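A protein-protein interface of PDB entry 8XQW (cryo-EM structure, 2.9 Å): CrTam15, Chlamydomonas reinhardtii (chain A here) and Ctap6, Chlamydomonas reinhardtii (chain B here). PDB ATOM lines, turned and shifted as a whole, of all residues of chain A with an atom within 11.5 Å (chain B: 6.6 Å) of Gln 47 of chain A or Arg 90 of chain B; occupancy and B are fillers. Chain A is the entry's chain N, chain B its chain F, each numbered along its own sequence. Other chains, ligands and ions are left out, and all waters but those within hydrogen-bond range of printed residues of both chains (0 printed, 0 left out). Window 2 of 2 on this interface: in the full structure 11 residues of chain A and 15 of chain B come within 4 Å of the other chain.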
ATOM      1  N   PRO A  38      -2.338   2.472   1.914  1.00  0.00           N
ATOM      2  CA  PRO A  38      -2.276   2.029   0.511  1.00  0.00           C
ATOM      3  C   PRO A  38      -1.513   0.736   0.276  1.00  0.00           C
ATOM      4  O   PRO A  38      -1.713   0.099  -0.766  1.00  0.00           O
ATOM      5  CB  PRO A  38      -1.590   3.211  -0.185  1.00  0.00           C
ATOM      6  CG  PRO A  38      -1.964   4.387   0.637  1.00  0.00           C
ATOM      7  CD  PRO A  38      -2.044   3.907   2.058  1.00  0.00           C
ATOM      8  N   SER A  39      -0.655   0.322   1.204  1.00  0.00           N
ATOM      9  CA  SER A  39       0.145  -0.877   0.990  1.00  0.00           C
ATOM     10  C   SER A  39      -0.662  -2.160   1.109  1.00  0.00           C
ATOM     11  O   SER A  39      -0.109  -3.240   0.877  1.00  0.00           O
ATOM     12  CB  SER A  39       1.311  -0.903   1.975  1.00  0.00           C
ATOM     13  OG  SER A  39       1.793   0.407   2.217  1.00  0.00           O
ATOM     14  N   LEU A  41      -3.211  -2.852  -0.793  1.00  0.00           N
ATOM     15  CA  LEU A  41      -3.851  -2.826  -2.096  1.00  0.00           C
ATOM     16  C   LEU A  41      -3.144  -3.768  -3.062  1.00  0.00           C
ATOM     17  O   LEU A  41      -2.022  -4.211  -2.796  1.00  0.00           O
ATOM     18  CB  LEU A  41      -3.834  -1.405  -2.667  1.00  0.00           C
ATOM     19  CG  LEU A  41      -4.795  -0.408  -2.020  1.00  0.00           C
ATOM     20  CD1 LEU A  41      -4.718   0.936  -2.723  1.00  0.00           C
ATOM     21  CD2 LEU A  41      -6.213  -0.947  -2.044  1.00  0.00           C
ATOM     22  N   PRO A  42      -3.776  -4.108  -4.183  1.00  0.00           N
ATOM     23  CA  PRO A  42      -3.087  -4.894  -5.213  1.00  0.00           C
ATOM     24  C   PRO A  42      -1.893  -4.144  -5.786  1.00  0.00           C
ATOM     25  O   PRO A  42      -1.583  -3.013  -5.410  1.00  0.00           O
ATOM     26  CB  PRO A  42      -4.171  -5.124  -6.268  1.00  0.00           C
ATOM     27  CG  PRO A  42      -5.443  -5.039  -5.511  1.00  0.00           C
ATOM     28  CD  PRO A  42      -5.222  -4.008  -4.447  1.00  0.00           C
ATOM     29  N   ALA A  43      -1.215  -4.807  -6.722  1.00  0.00           N
ATOM     30  CA  ALA A  43       0.100  -4.358  -7.165  1.00  0.00           C
ATOM     31  C   ALA A  43       0.056  -2.971  -7.798  1.00  0.00           C
ATOM     32  O   ALA A  43       0.618  -2.011  -7.261  1.00  0.00           O
ATOM     33  CB  ALA A  43       0.686  -5.373  -8.148  1.00  0.00           C
ATOM     34  N   GLY A  44      -0.609  -2.843  -8.941  1.00  0.00           N
ATOM     35  CA  GLY A  44      -0.485  -1.627  -9.718  1.00  0.00           C
ATOM     36  C   GLY A  44      -1.587  -0.616  -9.500  1.00  0.00           C
ATOM     37  O   GLY A  44      -1.763   0.299 -10.307  1.00  0.00           O
ATOM     38  N   VAL A  45      -2.324  -0.757  -8.406  1.00  0.00           N
ATOM     39  CA  VAL A  45      -3.450   0.122  -8.129  1.00  0.00           C
ATOM     40  C   VAL A  45      -2.983   1.520  -7.756  1.00  0.00           C
ATOM     41  O   VAL A  45      -3.624   2.516  -8.097  1.00  0.00           O
ATOM     42  CB  VAL A  45      -4.320  -0.503  -7.025  1.00  0.00           C
ATOM     43  CG1 VAL A  45      -5.427   0.429  -6.625  1.00  0.00           C
ATOM     44  CG2 VAL A  45      -4.882  -1.813  -7.508  1.00  0.00           C
ATOM     45  N   LEU A  46      -1.859   1.621  -7.060  1.00  0.00           N
ATOM     46  CA  LEU A  46      -1.328   2.925  -6.696  1.00  0.00           C
ATOM     47  C   LEU A  46      -0.707   3.599  -7.906  1.00  0.00           C
ATOM     48  O   LEU A  46       0.145   3.020  -8.586  1.00  0.00           O
ATOM     49  CB  LEU A  46      -0.295   2.788  -5.586  1.00  0.00           C
ATOM     50  CG  LEU A  46      -0.717   3.438  -4.273  1.00  0.00           C
ATOM     51  CD1 LEU A  46       0.387   3.319  -3.249  1.00  0.00           C
ATOM     52  CD2 LEU A  46      -1.073   4.894  -4.505  1.00  0.00           C
ATOM     53  N   GLN A  47      -1.173   4.818  -8.175  1.00  0.00           N
ATOM     54  CA  GLN A  47      -0.682   5.568  -9.354  1.00  0.00           C
ATOM     55  C   GLN A  47       0.461   6.472  -8.901  1.00  0.00           C
ATOM     56  O   GLN A  47       0.316   7.105  -7.845  1.00  0.00           O
ATOM     57  CB  GLN A  47      -1.850   6.305 -10.001  1.00  0.00           C
ATOM     58  CG  GLN A  47      -2.945   5.381 -10.519  1.00  0.00           C
ATOM     59  CD  GLN A  47      -2.596   4.771 -11.856  1.00  0.00           C
ATOM     60  OE1 GLN A  47      -2.853   5.353 -12.913  1.00  0.00           O
ATOM     61  NE2 GLN A  47      -2.000   3.589 -11.821  1.00  0.00           N
ATOM     62  N   THR A  48       1.550   6.504  -9.673  1.00  0.00           N
ATOM     63  CA  THR A  48       2.709   7.364  -9.370  1.00  0.00           C
ATOM     64  C   THR A  48       2.396   8.763  -9.825  1.00  0.00           C
ATOM     65  O   THR A  48       1.308   8.974 -10.382  1.00  0.00           O
ATOM     66  CB  THR A  48       3.926   6.819 -10.111  1.00  0.00           C
ATOM     67  OG1 THR A  48       4.046   7.600 -11.295  1.00  0.00           O
ATOM     68  CG2 THR A  48       3.768   5.362 -10.498  1.00  0.00           C
ATOM     69  N   ARG A  49       3.330   9.690  -9.639  1.00  0.00           N
ATOM     70  CA  ARG A  49       3.122  11.064 -10.146  1.00  0.00           C
ATOM     71  C   ARG A  49       3.332  11.044 -11.661  1.00  0.00           C
ATOM     72  O   ARG A  49       2.485  11.612 -12.378  1.00  0.00           O
ATOM     73  CB  ARG A  49       4.100  12.041  -9.498  1.00  0.00           C
ATOM     74  CG  ARG A  49       4.353  13.284 -10.339  1.00  0.00           C
ATOM     75  CD  ARG A  49       3.282  14.340 -10.142  1.00  0.00           C
ATOM     76  NE  ARG A  49       3.885  15.664  -9.952  1.00  0.00           N
ATOM     77  CZ  ARG A  49       5.019  15.881  -9.299  1.00  0.00           C
ATOM     78  NH1 ARG A  49       5.077  15.690  -7.993  1.00  0.00           N
ATOM     79  NH2 ARG A  49       6.091  16.290  -9.953  1.00  0.00           N
ATOM     80  N   GLU A  50       4.400  10.392 -12.121  1.00  0.00           N
ATOM     81  CA  GLU A  50       4.648  10.280 -13.579  1.00  0.00           C
ATOM     82  C   GLU A  50       3.318   9.966 -14.262  1.00  0.00           C
ATOM     83  O   GLU A  50       2.869  10.775 -15.095  1.00  0.00           O
ATOM     84  CB  GLU A  50       5.635   9.149 -13.848  1.00  0.00           C
ATOM     85  CG  GLU A  50       5.765   8.790 -15.324  1.00  0.00           C
ATOM     86  CD  GLU A  50       6.697   9.706 -16.093  1.00  0.00           C
ATOM     87  OE1 GLU A  50       7.644  10.238 -15.479  1.00  0.00           O
ATOM     88  OE2 GLU A  50       6.474   9.888 -17.308  1.00  0.00           O
ATOM     89  N   GLN A  51       2.716   8.835 -13.898  1.00  0.00           N
ATOM     90  CA  GLN A  51       1.420   8.435 -14.481  1.00  0.00           C
ATOM     91  C   GLN A  51       0.393   9.546 -14.281  1.00  0.00           C
ATOM     92  O   GLN A  51       0.035  10.191 -15.271  1.00  0.00           O
ATOM     93  CB  GLN A  51       0.945   7.190 -13.744  1.00  0.00           C
ATOM     94  CG  GLN A  51       1.330   5.876 -14.411  1.00  0.00           C
ATOM     95  CD  GLN A  51       1.111   4.684 -13.508  1.00  0.00           C
ATOM     96  OE1 GLN A  51       0.953   4.818 -12.291  1.00  0.00           O
ATOM     97  NE2 GLN A  51       1.099   3.499 -14.098  1.00  0.00           N
ATOM     98  N   LEU A  52      -0.042   9.785 -13.050  1.00  0.00           N
ATOM     99  CA  LEU A  52      -1.146  10.744 -12.785  1.00  0.00           C
ATOM    100  C   LEU A  52      -1.005  12.063 -13.559  1.00  0.00           C
ATOM    101  O   LEU A  52      -2.040  12.727 -13.729  1.00  0.00           O
ATOM    102  CB  LEU A  52      -1.223  10.991 -11.283  1.00  0.00           C
ATOM    103  CG  LEU A  52      -2.035   9.972 -10.482  1.00  0.00           C
ATOM    104  CD1 LEU A  52      -2.619  10.626  -9.245  1.00  0.00           C
ATOM    105  CD2 LEU A  52      -3.133   9.394 -11.352  1.00  0.00           C
ATOM    106  N   LYS A  53       0.198  12.456 -13.972  1.00  0.00           N
ATOM    107  CA  LYS A  53       0.348  13.773 -14.642  1.00  0.00           C
ATOM    108  C   LYS A  53      -0.041  13.597 -16.105  1.00  0.00           C
ATOM    109  O   LYS A  53      -0.751  14.467 -16.631  1.00  0.00           O
ATOM    110  CB  LYS A  53       1.781  14.276 -14.471  1.00  0.00           C
ATOM    111  CG  LYS A  53       2.569  14.593 -15.731  1.00  0.00           C
ATOM    112  CD  LYS A  53       4.035  14.200 -15.603  1.00  0.00           C
ATOM    113  CE  LYS A  53       4.452  14.056 -14.174  1.00  0.00           C
ATOM    114  NZ  LYS A  53       4.803  15.341 -13.563  1.00  0.00           N
ATOM    115  N   GLN A  54       0.397  12.509 -16.722  1.00  0.00           N
ATOM    116  CA  GLN A  54       0.025  12.180 -18.091  1.00  0.00           C
ATOM    117  C   GLN A  54      -1.485  12.082 -18.245  1.00  0.00           C
ATOM    118  O   GLN A  54      -2.039  12.487 -19.274  1.00  0.00           O
ATOM    119  CB  GLN A  54       0.695  10.873 -18.488  1.00  0.00           C
ATOM    120  CG  GLN A  54       0.517  10.492 -19.922  1.00  0.00           C
ATOM    121  CD  GLN A  54       1.333   9.272 -20.269  1.00  0.00           C
ATOM    122  OE1 GLN A  54       1.210   8.233 -19.626  1.00  0.00           O
ATOM    123  NE2 GLN A  54       2.178   9.392 -21.283  1.00  0.00           N
ATOM    124  N   ALA A  55      -2.169  11.545 -17.237  1.00  0.00           N
ATOM    125  CA  ALA A  55      -3.620  11.469 -17.304  1.00  0.00           C
ATOM    126  C   ALA A  55      -4.240  12.857 -17.314  1.00  0.00           C
ATOM    127  O   ALA A  55      -5.206  13.111 -18.041  1.00  0.00           O
ATOM    128  CB  ALA A  55      -4.151  10.650 -16.134  1.00  0.00           C
ATOM    129  N   GLN A  56      -3.689  13.778 -16.526  1.00  0.00           N
ATOM    130  CA  GLN A  56      -4.195  15.145 -16.559  1.00  0.00           C
ATOM    131  C   GLN A  56      -3.920  15.793 -17.909  1.00  0.00           C
ATOM    132  O   GLN A  56      -4.747  16.557 -18.427  1.00  0.00           O
ATOM    133  CB  GLN A  56      -3.573  15.958 -15.432  1.00  0.00           C
ATOM    134  CG  GLN A  56      -4.195  17.316 -15.262  1.00  0.00           C
ATOM    135  CD  GLN A  56      -5.694  17.240 -15.126  1.00  0.00           C
ATOM    136  OE1 GLN A  56      -6.214  16.482 -14.313  1.00  0.00           O
ATOM    137  NE2 GLN A  56      -6.402  18.022 -15.931  1.00  0.00           N
ATOM    138  N   ARG A  57      -2.767  15.483 -18.502  1.00  0.00           N
ATOM    139  CA  ARG A  57      -2.451  16.005 -19.826  1.00  0.00           C
ATOM    140  C   ARG A  57      -3.473  15.547 -20.857  1.00  0.00           C
ATOM    141  O   ARG A  57      -3.995  16.355 -21.638  1.00  0.00           O
ATOM    142  CB  ARG A  57      -1.050  15.569 -20.229  1.00  0.00           C
ATOM    143  CG  ARG A  57      -0.723  15.807 -21.679  1.00  0.00           C
ATOM    144  CD  ARG A  57       0.763  15.685 -21.906  1.00  0.00           C
ATOM    145  NE  ARG A  57       1.502  16.088 -20.719  1.00  0.00           N
ATOM    146  CZ  ARG A  57       2.266  15.272 -20.003  1.00  0.00           C
ATOM    147  NH1 ARG A  57       2.395  14.002 -20.360  1.00  0.00           N
ATOM    148  NH2 ARG A  57       2.900  15.726 -18.932  1.00  0.00           N
ATOM    149  N   ASP A  58      -3.762  14.246 -20.881  1.00  0.00           N
ATOM    150  CA  ASP A  58      -4.792  13.737 -21.776  1.00  0.00           C
ATOM    151  C   ASP A  58      -6.161  14.335 -21.506  1.00  0.00           C
ATOM    152  O   ASP A  58      -6.898  14.594 -22.459  1.00  0.00           O
ATOM    153  CB  ASP A  58      -4.900  12.221 -21.683  1.00  0.00           C
ATOM    154  CG  ASP A  58      -3.581  11.538 -21.871  1.00  0.00           C
ATOM    155  OD1 ASP A  58      -2.670  12.169 -22.439  1.00  0.00           O
ATOM    156  OD2 ASP A  58      -3.456  10.367 -21.456  1.00  0.00           O
ATOM    157  N   ILE A  59      -6.522  14.551 -20.240  1.00  0.00           N
ATOM    158  CA  ILE A  59      -7.811  15.163 -19.937  1.00  0.00           C
ATOM    159  C   ILE A  59      -7.900  16.548 -20.563  1.00  0.00           C
ATOM    160  O   ILE A  59      -8.905  16.904 -21.190  1.00  0.00           O
ATOM    161  CB  ILE A  59      -8.033  15.216 -18.419  1.00  0.00           C
ATOM    162  CG1 ILE A  59      -8.287  13.816 -17.880  1.00  0.00           C
ATOM    163  CG2 ILE A  59      -9.204  16.106 -18.094  1.00  0.00           C
ATOM    164  CD1 ILE A  59      -8.492  13.774 -16.396  1.00  0.00           C
ATOM    165  N   PRO B  82      -5.145   8.771  -1.732  1.00  0.00           N
ATOM    166  CA  PRO B  82      -4.482   8.670  -3.033  1.00  0.00           C
ATOM    167  C   PRO B  82      -5.391   8.041  -4.075  1.00  0.00           C
ATOM    168  O   PRO B  82      -6.178   7.140  -3.786  1.00  0.00           O
ATOM    169  CB  PRO B  82      -3.281   7.766  -2.739  1.00  0.00           C
ATOM    170  CG  PRO B  82      -3.743   6.922  -1.617  1.00  0.00           C
ATOM    171  CD  PRO B  82      -4.557   7.840  -0.757  1.00  0.00           C
ATOM    172  N   GLU B  83      -5.261   8.525  -5.307  1.00  0.00           N
ATOM    173  CA  GLU B  83      -6.082   8.014  -6.393  1.00  0.00           C
ATOM    174  C   GLU B  83      -5.633   6.616  -6.801  1.00  0.00           C
ATOM    175  O   GLU B  83      -4.461   6.251  -6.680  1.00  0.00           O
ATOM    176  CB  GLU B  83      -6.026   8.950  -7.596  1.00  0.00           C
ATOM    177  CG  GLU B  83      -7.183   8.770  -8.562  1.00  0.00           C
ATOM    178  CD  GLU B  83      -7.630  10.079  -9.188  1.00  0.00           C
ATOM    179  OE1 GLU B  83      -6.780  10.977  -9.357  1.00  0.00           O
ATOM    180  OE2 GLU B  83      -8.831  10.213  -9.504  1.00  0.00           O
ATOM    181  N   LYS B  84      -6.585   5.835  -7.298  1.00  0.00           N
ATOM    182  CA  LYS B  84      -6.366   4.431  -7.595  1.00  0.00           C
ATOM    183  C   LYS B  84      -6.860   4.108  -8.994  1.00  0.00           C
ATOM    184  O   LYS B  84      -7.720   4.793  -9.549  1.00  0.00           O
ATOM    185  CB  LYS B  84      -7.072   3.543  -6.573  1.00  0.00           C
ATOM    186  CG  LYS B  84      -6.451   3.598  -5.207  1.00  0.00           C
ATOM    187  CD  LYS B  84      -7.423   3.130  -4.163  1.00  0.00           C
ATOM    188  CE  LYS B  84      -8.387   4.228  -3.822  1.00  0.00           C
ATOM    189  NZ  LYS B  84      -7.652   5.424  -3.354  1.00  0.00           N
ATOM    190  N   ASN B  85      -6.309   3.037  -9.553  1.00  0.00           N
ATOM    191  CA  ASN B  85      -6.643   2.579 -10.894  1.00  0.00           C
ATOM    192  C   ASN B  85      -6.886   1.081 -10.823  1.00  0.00           C
ATOM    193  O   ASN B  85      -5.950   0.291 -10.973  1.00  0.00           O
ATOM    194  CB  ASN B  85      -5.527   2.917 -11.879  1.00  0.00           C
ATOM    195  CG  ASN B  85      -5.801   2.414 -13.282  1.00  0.00           C
ATOM    196  OD1 ASN B  85      -5.842   1.212 -13.532  1.00  0.00           O
ATOM    197  ND2 ASN B  85      -5.998   3.340 -14.208  1.00  0.00           N
ATOM    198  N   TYR B  86      -8.132   0.690 -10.590  1.00  0.00           N
ATOM    199  CA  TYR B  86      -8.489  -0.712 -10.450  1.00  0.00           C
ATOM    200  C   TYR B  86      -8.521  -1.446 -11.775  1.00  0.00           C
ATOM    201  O   TYR B  86      -8.865  -2.630 -11.801  1.00  0.00           O
ATOM    202  CB  TYR B  86      -9.844  -0.842  -9.762  1.00  0.00           C
ATOM    203  CG  TYR B  86      -9.825  -0.459  -8.310  1.00  0.00           C
ATOM    204  CD1 TYR B  86      -9.274  -1.301  -7.358  1.00  0.00           C
ATOM    205  CD2 TYR B  86     -10.358   0.747  -7.889  1.00  0.00           C
ATOM    206  CE1 TYR B  86      -9.256  -0.954  -6.030  1.00  0.00           C
ATOM    207  CE2 TYR B  86     -10.344   1.103  -6.564  1.00  0.00           C
ATOM    208  CZ  TYR B  86      -9.793   0.250  -5.638  1.00  0.00           C
ATOM    209  OH  TYR B  86      -9.780   0.610  -4.312  1.00  0.00           O
ATOM    210  N   GLY B  87      -8.184  -0.786 -12.862  1.00  0.00           N
ATOM    211  CA  GLY B  87      -8.290  -1.373 -14.189  1.00  0.00           C
ATOM    212  C   GLY B  87      -9.635  -1.137 -14.824  1.00  0.00           C
ATOM    213  O   GLY B  87      -9.718  -0.734 -15.981  1.00  0.00           O
ATOM    214  N   SER B  88     -10.703  -1.378 -14.068  1.00  0.00           N
ATOM    215  CA  SER B  88     -12.062  -1.208 -14.546  1.00  0.00           C
ATOM    216  C   SER B  88     -12.617   0.166 -14.224  1.00  0.00           C
ATOM    217  O   SER B  88     -13.380   0.724 -15.012  1.00  0.00           O
ATOM    218  CB  SER B  88     -12.963  -2.277 -13.943  1.00  0.00           C
ATOM    219  OG  SER B  88     -14.128  -2.441 -14.721  1.00  0.00           O
ATOM    220  N   LEU B  89     -12.258   0.720 -13.073  1.00  0.00           N
ATOM    221  CA  LEU B  89     -12.670   2.058 -12.693  1.00  0.00           C
ATOM    222  C   LEU B  89     -11.483   2.782 -12.086  1.00  0.00           C
ATOM    223  O   LEU B  89     -10.516   2.159 -11.651  1.00  0.00           O
ATOM    224  CB  LEU B  89     -13.828   2.038 -11.703  1.00  0.00           C
ATOM    225  CG  LEU B  89     -15.128   1.447 -12.230  1.00  0.00           C
ATOM    226  CD1 LEU B  89     -16.153   1.335 -11.134  1.00  0.00           C
ATOM    227  CD2 LEU B  89     -15.647   2.308 -13.342  1.00  0.00           C
ATOM    228  N   ARG B  90     -11.556   4.104 -12.073  1.00  0.00           N
ATOM    229  CA  ARG B  90     -10.522   4.925 -11.475  1.00  0.00           C
ATOM    230  C   ARG B  90     -11.167   5.961 -10.571  1.00  0.00           C
ATOM    231  O   ARG B  90     -12.290   6.407 -10.817  1.00  0.00           O
ATOM    232  CB  ARG B  90      -9.669   5.612 -12.538  1.00  0.00           C
ATOM    233  CG  ARG B  90     -10.343   6.794 -13.188  1.00  0.00           C
ATOM    234  CD  ARG B  90      -9.341   7.746 -13.796  1.00  0.00           C
ATOM    235  NE  ARG B  90      -8.209   7.044 -14.381  1.00  0.00           N
ATOM    236  CZ  ARG B  90      -6.942   7.301 -14.081  1.00  0.00           C
ATOM    237  NH1 ARG B  90      -5.974   6.614 -14.661  1.00  0.00           N
ATOM    238  NH2 ARG B  90      -6.644   8.247 -13.204  1.00  0.00           N
ATOM    239  N   GLY B  91     -10.453   6.326  -9.515  1.00  0.00           N
ATOM    240  CA  GLY B  91     -10.964   7.266  -8.536  1.00  0.00           C
ATOM    241  C   GLY B  91     -10.667   6.820  -7.122  1.00  0.00           C
ATOM    242  O   GLY B  91      -9.677   6.127  -6.885  1.00  0.00           O
ATOM    243  N   GLY B  92     -11.514   7.202  -6.175  1.00  0.00           N
ATOM    244  CA  GLY B  92     -11.316   6.781  -4.803  1.00  0.00           C
ATOM    245  C   GLY B  92     -10.558   7.765  -3.941  1.00  0.00           C
ATOM    246  O   GLY B  92      -9.718   7.355  -3.134  1.00  0.00           O
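Of the printed residues of chain B, Gln 47 of chain A touches Glu 83, Asn 85 and Arg 90.
Arg 90 of chain B touches one residue of chain A.
Glu 83 of chain B touches just one residue of chain A: Gln 47 (3.9 Å).
Of chain A, only Val 45 (3.1 Å) and Gln 47 (3.5 Å) come within 4 Å of Asn 85 of chain B.
No residue of chain A comes within 4 Å of Gly 87 of chain B.
No residue of chain A comes within 4 Å of Gly 91 of chain B.
Printed residues of chain B within 4 Å of Leu 41 of chain A: Lys 84.
Of the printed residues of chain A, Pro 82 of chain B touches Pro 38.
Of the printed residues of chain B, Val 45 of chain A touches Lys 84 and Asn 85.
Of the printed residues of chain B, Pro 38 of chain A touches Pro 82 (3.8 Å).
Gln 51 of chain A touches none of the printed residues of chain B.
The nearest residue of chain B that does not touch Gln 47 of chain A is Lys 84 of chain B (4.4 Å).
The nearest printed residue of chain A that does not touch Lys 84 of chain B is Gln 47 of chain A (4.4 Å).
CG of Pro 38 of chain A touches CG of Pro 82 of chain B, 3.8 Å away.
CD1 of Leu 41 of chain A touches CD of Lys 84 of chain B, at 3.8 Å.
Val 45 of chain A touches Lys 84 of chain B (O to CA, 3.4 Å).
N of Gln 47 of chain A touches O of Glu 83 of chain B (3.9 Å).
CD of Gln 47 of chain A touches CB of Asn 85 of chain B (3.5 Å).
Arg 90 of chain B touches Gln 47 of chain A (NH1 to OE1, 3.8 Å).
The backbone carbonyl oxygen (O) of Val 45 of chain A is in hydrogen-bond range of the backbone NH (N) of Asn 85 of chain B (3.1 Å).
Hydrophobic or aromatic side chains of chain A that line the printed part of chain B: Pro 38, Leu 41 and Val 45.
Of the 11 printed residues of chain B, 5 touch a printed residue of chain A.
NE2 of Gln 47 of chain A is in hydrogen-bond range of OE1 of Gln 51 of chain A.
The backbone NH (N) of Lys 84 of chain B is in hydrogen-bond range of the backbone carbonyl oxygen (O) of Gly 91 of chain B, 3.1 Å away.
The backbone carbonyl oxygen (O) of Gly 92 of chain B lies within hydrogen-bond range of the side-chain amino group (NZ) of Lys 84 of chain B (2.8 Å).
The side-chain amide oxygen of Asn 85 of chain B lies close to the backbone NH of Gly 87 of chain B, at 3.2 Å.
The side-chain amide nitrogen (ND2) of Asn 85 of chain B sits close to the guanidinium group (NH1) of Arg 90 of chain B, at 3.3 Å.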
